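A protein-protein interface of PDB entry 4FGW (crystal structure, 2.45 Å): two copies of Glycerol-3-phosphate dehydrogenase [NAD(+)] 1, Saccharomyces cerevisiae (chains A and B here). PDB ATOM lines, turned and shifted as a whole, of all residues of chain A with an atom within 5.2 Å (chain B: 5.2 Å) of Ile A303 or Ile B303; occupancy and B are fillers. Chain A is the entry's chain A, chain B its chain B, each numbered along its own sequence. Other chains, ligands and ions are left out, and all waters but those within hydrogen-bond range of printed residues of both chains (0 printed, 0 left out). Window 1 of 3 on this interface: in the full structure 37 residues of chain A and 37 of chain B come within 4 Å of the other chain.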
ATOM      1  N   ALA A 266      24.603  12.858 -18.912  1.00  0.00           N
ATOM      2  CA  ALA A 266      23.297  12.519 -19.498  1.00  0.00           C
ATOM      3  C   ALA A 266      22.266  13.626 -19.216  1.00  0.00           C
ATOM      4  O   ALA A 266      21.455  13.927 -20.091  1.00  0.00           O
ATOM      5  CB  ALA A 266      22.811  11.193 -18.943  1.00  0.00           C
ATOM      6  N   GLN A 269      22.972  16.516 -21.569  1.00  0.00           N
ATOM      7  CA  GLN A 269      22.491  16.097 -22.887  1.00  0.00           C
ATOM      8  C   GLN A 269      20.978  16.268 -22.985  1.00  0.00           C
ATOM      9  O   GLN A 269      20.488  16.755 -24.004  1.00  0.00           O
ATOM     10  CB  GLN A 269      22.901  14.655 -23.191  1.00  0.00           C
ATOM     11  CG  GLN A 269      24.371  14.557 -23.569  1.00  0.00           C
ATOM     12  CD  GLN A 269      24.880  13.148 -23.669  1.00  0.00           C
ATOM     13  OE1 GLN A 269      25.645  12.687 -22.825  1.00  0.00           O
ATOM     14  NE2 GLN A 269      24.517  12.456 -24.729  1.00  0.00           N
ATOM     15  N   VAL A 299      19.125  13.785 -31.900  1.00  0.00           N
ATOM     16  CA  VAL A 299      19.542  13.027 -30.717  1.00  0.00           C
ATOM     17  C   VAL A 299      20.831  12.180 -30.890  1.00  0.00           C
ATOM     18  O   VAL A 299      21.729  12.263 -30.041  1.00  0.00           O
ATOM     19  CB  VAL A 299      18.347  12.239 -30.092  1.00  0.00           C
ATOM     20  CG1 VAL A 299      17.917  11.049 -30.958  1.00  0.00           C
ATOM     21  CG2 VAL A 299      18.660  11.787 -28.666  1.00  0.00           C
ATOM     22  N   ALA A 300      20.927  11.393 -31.983  1.00  0.00           N
ATOM     23  CA  ALA A 300      22.088  10.523 -32.234  1.00  0.00           C
ATOM     24  C   ALA A 300      23.377  11.342 -32.411  1.00  0.00           C
ATOM     25  O   ALA A 300      24.406  11.008 -31.807  1.00  0.00           O
ATOM     26  CB  ALA A 300      21.842   9.635 -33.449  1.00  0.00           C
ATOM     27  N   ASP A 301      23.302  12.454 -33.166  1.00  0.00           N
ATOM     28  CA  ASP A 301      24.467  13.307 -33.360  1.00  0.00           C
ATOM     29  C   ASP A 301      24.905  13.973 -32.064  1.00  0.00           C
ATOM     30  O   ASP A 301      26.106  14.096 -31.811  1.00  0.00           O
ATOM     31  CB  ASP A 301      24.268  14.307 -34.500  1.00  0.00           C
ATOM     32  CG  ASP A 301      25.566  14.680 -35.185  1.00  0.00           C
ATOM     33  OD1 ASP A 301      26.602  14.078 -34.858  1.00  0.00           O
ATOM     34  OD2 ASP A 301      25.544  15.575 -36.047  1.00  0.00           O
ATOM     35  N   LEU A 302      23.930  14.335 -31.217  1.00  0.00           N
ATOM     36  CA  LEU A 302      24.191  14.894 -29.893  1.00  0.00           C
ATOM     37  C   LEU A 302      24.913  13.847 -29.009  1.00  0.00           C
ATOM     38  O   LEU A 302      25.935  14.159 -28.403  1.00  0.00           O
ATOM     39  CB  LEU A 302      22.867  15.339 -29.244  1.00  0.00           C
ATOM     40  CG  LEU A 302      22.962  15.987 -27.856  1.00  0.00           C
ATOM     41  CD1 LEU A 302      23.659  17.352 -27.927  1.00  0.00           C
ATOM     42  CD2 LEU A 302      21.595  16.117 -27.221  1.00  0.00           C
ATOM     43  N   ILE A 303      24.379  12.606 -28.960  1.00  0.00           N
ATOM     44  CA  ILE A 303      24.941  11.505 -28.177  1.00  0.00           C
ATOM     45  C   ILE A 303      26.405  11.234 -28.548  1.00  0.00           C
ATOM     46  O   ILE A 303      27.259  11.255 -27.666  1.00  0.00           O
ATOM     47  CB  ILE A 303      24.040  10.227 -28.218  1.00  0.00           C
ATOM     48  CG1 ILE A 303      22.710  10.478 -27.472  1.00  0.00           C
ATOM     49  CG2 ILE A 303      24.780   8.995 -27.623  1.00  0.00           C
ATOM     50  CD1 ILE A 303      21.586   9.409 -27.711  1.00  0.00           C
ATOM     51  N   THR A 304      26.693  11.018 -29.836  1.00  0.00           N
ATOM     52  CA  THR A 304      28.058  10.745 -30.299  1.00  0.00           C
ATOM     53  C   THR A 304      29.059  11.855 -29.977  1.00  0.00           C
ATOM     54  O   THR A 304      30.185  11.560 -29.570  1.00  0.00           O
ATOM     55  CB  THR A 304      28.083  10.250 -31.756  1.00  0.00           C
ATOM     56  OG1 THR A 304      29.346   9.626 -31.998  1.00  0.00           O
ATOM     57  CG2 THR A 304      27.839  11.366 -32.796  1.00  0.00           C
ATOM     58  N   THR A 305      28.632  13.121 -30.144  1.00  0.00           N
ATOM     59  CA  THR A 305      29.441  14.313 -29.901  1.00  0.00           C
ATOM     60  C   THR A 305      29.778  14.452 -28.418  1.00  0.00           C
ATOM     61  O   THR A 305      30.922  14.730 -28.070  1.00  0.00           O
ATOM     62  CB  THR A 305      28.751  15.546 -30.501  1.00  0.00           C
ATOM     63  OG1 THR A 305      28.473  15.289 -31.881  1.00  0.00           O
ATOM     64  CG2 THR A 305      29.592  16.808 -30.373  1.00  0.00           C
ATOM     65  N   CYS A 306      28.790  14.231 -27.554  1.00  0.00           N
ATOM     66  CA  CYS A 306      28.969  14.300 -26.114  1.00  0.00           C
ATOM     67  C   CYS A 306      29.737  13.093 -25.542  1.00  0.00           C
ATOM     68  O   CYS A 306      30.343  13.215 -24.482  1.00  0.00           O
ATOM     69  CB  CYS A 306      27.626  14.504 -25.428  1.00  0.00           C
ATOM     70  SG  CYS A 306      26.787  16.044 -25.891  1.00  0.00           S
ATOM     71  N   ALA A 307      29.753  11.954 -26.263  1.00  0.00           N
ATOM     72  CA  ALA A 307      30.477  10.738 -25.869  1.00  0.00           C
ATOM     73  C   ALA A 307      31.989  10.898 -26.073  1.00  0.00           C
ATOM     74  O   ALA A 307      32.765  10.536 -25.191  1.00  0.00           O
ATOM     75  CB  ALA A 307      29.962   9.532 -26.647  1.00  0.00           C
ATOM     76  N   GLY A 308      32.385  11.435 -27.224  1.00  0.00           N
ATOM     77  CA  GLY A 308      33.781  11.652 -27.584  1.00  0.00           C
ATOM     78  C   GLY A 308      33.929  12.603 -28.752  1.00  0.00           C
ATOM     79  O   GLY A 308      33.126  12.575 -29.691  1.00  0.00           O
ATOM     80  N   ALA B 266      25.265   5.336 -30.909  1.00  0.00           N
ATOM     81  CA  ALA B 266      24.309   6.449 -30.942  1.00  0.00           C
ATOM     82  C   ALA B 266      23.093   6.109 -31.830  1.00  0.00           C
ATOM     83  O   ALA B 266      21.973   6.472 -31.483  1.00  0.00           O
ATOM     84  CB  ALA B 266      25.001   7.705 -31.442  1.00  0.00           C
ATOM     85  N   GLN B 269      20.836   3.762 -29.884  1.00  0.00           N
ATOM     86  CA  GLN B 269      20.150   4.594 -28.892  1.00  0.00           C
ATOM     87  C   GLN B 269      18.981   5.343 -29.525  1.00  0.00           C
ATOM     88  O   GLN B 269      17.906   5.407 -28.934  1.00  0.00           O
ATOM     89  CB  GLN B 269      21.123   5.562 -28.216  1.00  0.00           C
ATOM     90  CG  GLN B 269      22.004   4.855 -27.199  1.00  0.00           C
ATOM     91  CD  GLN B 269      23.121   5.709 -26.668  1.00  0.00           C
ATOM     92  OE1 GLN B 269      24.299   5.499 -26.973  1.00  0.00           O
ATOM     93  NE2 GLN B 269      22.784   6.641 -25.811  1.00  0.00           N
ATOM     94  N   VAL B 299      15.125   9.798 -22.175  1.00  0.00           N
ATOM     95  CA  VAL B 299      16.378   9.993 -22.909  1.00  0.00           C
ATOM     96  C   VAL B 299      17.665   9.968 -22.044  1.00  0.00           C
ATOM     97  O   VAL B 299      18.606   9.252 -22.399  1.00  0.00           O
ATOM     98  CB  VAL B 299      16.301  11.215 -23.879  1.00  0.00           C
ATOM     99  CG1 VAL B 299      16.313  12.548 -23.125  1.00  0.00           C
ATOM    100  CG2 VAL B 299      17.409  11.172 -24.936  1.00  0.00           C
ATOM    101  N   ALA B 300      17.691  10.720 -20.915  1.00  0.00           N
ATOM    102  CA  ALA B 300      18.865  10.797 -20.036  1.00  0.00           C
ATOM    103  C   ALA B 300      19.206   9.446 -19.433  1.00  0.00           C
ATOM    104  O   ALA B 300      20.371   9.035 -19.461  1.00  0.00           O
ATOM    105  CB  ALA B 300      18.652  11.839 -18.947  1.00  0.00           C
ATOM    106  N   ASP B 301      18.185   8.725 -18.945  1.00  0.00           N
ATOM    107  CA  ASP B 301      18.405   7.398 -18.371  1.00  0.00           C
ATOM    108  C   ASP B 301      18.883   6.391 -19.412  1.00  0.00           C
ATOM    109  O   ASP B 301      19.736   5.569 -19.102  1.00  0.00           O
ATOM    110  CB  ASP B 301      17.186   6.901 -17.585  1.00  0.00           C
ATOM    111  CG  ASP B 301      17.534   5.877 -16.526  1.00  0.00           C
ATOM    112  OD1 ASP B 301      18.752   5.635 -16.291  1.00  0.00           O
ATOM    113  OD2 ASP B 301      16.609   5.306 -15.944  1.00  0.00           O
ATOM    114  N   LEU B 302      18.389   6.507 -20.658  1.00  0.00           N
ATOM    115  CA  LEU B 302      18.835   5.697 -21.788  1.00  0.00           C
ATOM    116  C   LEU B 302      20.330   5.983 -22.076  1.00  0.00           C
ATOM    117  O   LEU B 302      21.129   5.049 -22.188  1.00  0.00           O
ATOM    118  CB  LEU B 302      17.974   6.008 -23.040  1.00  0.00           C
ATOM    119  CG  LEU B 302      18.278   5.200 -24.311  1.00  0.00           C
ATOM    120  CD1 LEU B 302      17.940   3.726 -24.136  1.00  0.00           C
ATOM    121  CD2 LEU B 302      17.552   5.774 -25.508  1.00  0.00           C
ATOM    122  N   ILE B 303      20.700   7.276 -22.178  1.00  0.00           N
ATOM    123  CA  ILE B 303      22.076   7.711 -22.450  1.00  0.00           C
ATOM    124  C   ILE B 303      23.057   7.144 -21.422  1.00  0.00           C
ATOM    125  O   ILE B 303      24.030   6.482 -21.812  1.00  0.00           O
ATOM    126  CB  ILE B 303      22.186   9.262 -22.637  1.00  0.00           C
ATOM    127  CG1 ILE B 303      21.460   9.707 -23.935  1.00  0.00           C
ATOM    128  CG2 ILE B 303      23.662   9.722 -22.640  1.00  0.00           C
ATOM    129  CD1 ILE B 303      21.204  11.238 -24.081  1.00  0.00           C
ATOM    130  N   THR B 304      22.791   7.368 -20.122  1.00  0.00           N
ATOM    131  CA  THR B 304      23.674   6.889 -19.049  1.00  0.00           C
ATOM    132  C   THR B 304      23.844   5.371 -19.028  1.00  0.00           C
ATOM    133  O   THR B 304      24.952   4.896 -18.818  1.00  0.00           O
ATOM    134  CB  THR B 304      23.316   7.509 -17.699  1.00  0.00           C
ATOM    135  OG1 THR B 304      24.425   7.356 -16.819  1.00  0.00           O
ATOM    136  CG2 THR B 304      22.048   6.903 -17.071  1.00  0.00           C
ATOM    137  N   THR B 305      22.751   4.624 -19.266  1.00  0.00           N
ATOM    138  CA  THR B 305      22.714   3.159 -19.281  1.00  0.00           C
ATOM    139  C   THR B 305      23.530   2.611 -20.440  1.00  0.00           C
ATOM    140  O   THR B 305      24.301   1.672 -20.252  1.00  0.00           O
ATOM    141  CB  THR B 305      21.256   2.673 -19.244  1.00  0.00           C
ATOM    142  OG1 THR B 305      20.619   3.256 -18.097  1.00  0.00           O
ATOM    143  CG2 THR B 305      21.133   1.163 -19.170  1.00  0.00           C
ATOM    144  N   CYS B 306      23.389   3.218 -21.620  1.00  0.00           N
ATOM    145  CA  CYS B 306      24.131   2.824 -22.812  1.00  0.00           C
ATOM    146  C   CYS B 306      25.600   3.245 -22.764  1.00  0.00           C
ATOM    147  O   CYS B 306      26.419   2.613 -23.421  1.00  0.00           O
ATOM    148  CB  CYS B 306      23.427   3.316 -24.070  1.00  0.00           C
ATOM    149  SG  CYS B 306      21.757   2.639 -24.288  1.00  0.00           S
ATOM    150  N   ALA B 307      25.943   4.270 -21.960  1.00  0.00           N
ATOM    151  CA  ALA B 307      27.323   4.757 -21.784  1.00  0.00           C
ATOM    152  C   ALA B 307      28.153   3.809 -20.920  1.00  0.00           C
ATOM    153  O   ALA B 307      29.290   3.494 -21.272  1.00  0.00           O
ATOM    154  CB  ALA B 307      27.323   6.158 -21.179  1.00  0.00           C
ATOM    155  N   GLY B 308      27.579   3.357 -19.808  1.00  0.00           N
ATOM    156  CA  GLY B 308      28.235   2.450 -18.872  1.00  0.00           C
ATOM    157  C   GLY B 308      27.250   1.793 -17.931  1.00  0.00           C
ATOM    158  O   GLY B 308      26.290   2.429 -17.484  1.00  0.00           O
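Among the printed residues, pairs that only touch across the chains: Ala A266 with Ala B300 (3.3 Å), Ala A300 with Ala B266 (3.4 Å), Gln A269 with Ile B303 (3.5 Å), Ile A303 with Gln B269 (3.6 Å), Ile A303 with Ile B303 (3.8 Å), Ala A266 with Thr B304 (3.9 Å) and Val A299 with Val B299 (3.98 Å).
Of chain B, only Gln B269 (3.6 Å) and Ile B303 (3.8 Å) come within 4 Å of Ile A303.
Ile B303 touches just these residues of chain A: Gln A269 and Ile A303.
Printed residues of chain A within 4 Å of Val B299: Val A299.
Of the printed residues of chain A, Ala B300 touches Ala A266 (3.3 Å).
Of the printed residues of chain B, Ala A266 touches Ala B300 and Thr B304.
Leu B302 touches none of the printed residues of chain A.
The nearest residue of chain B that does not touch Ile A303 is Ala B266 (4.04 Å).
The nearest residue of chain A that does not touch Ile B303 is Ala A266 (4.1 Å).
Of the 12 printed residues of chain A, 5 touch a printed residue of chain B.
Printed residues of chain A that touch a printed residue of chain B: Ala A266, Gln A269, Val A299, Ala A300 and Ile A303.
Hydrophobic or aromatic side chains of chain B within 4 Å of the printed part of chain A: Ala B266, Val B299, Ala B300 and Ile B303.
Among the printed residues, no Asp or Glu carboxylate lies within 4 Å of a Lys or Arg side-chain nitrogen of the other chain.
Ala A266 touches Ala B300, and with the chains exchanged Ala A300 touches Ala B266.
Ala A266 touches Thr B304, but with the chains exchanged Thr A304 does not touch Ala B266 (4.01 Å).
Val A299 touches its own counterpart, Val B299.
Ile B303 touches its own counterpart, Ile A303.
Of the 7 pairs that touch across the chains among the printed residues, 6 have their exchanged pair printed and touching as well.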
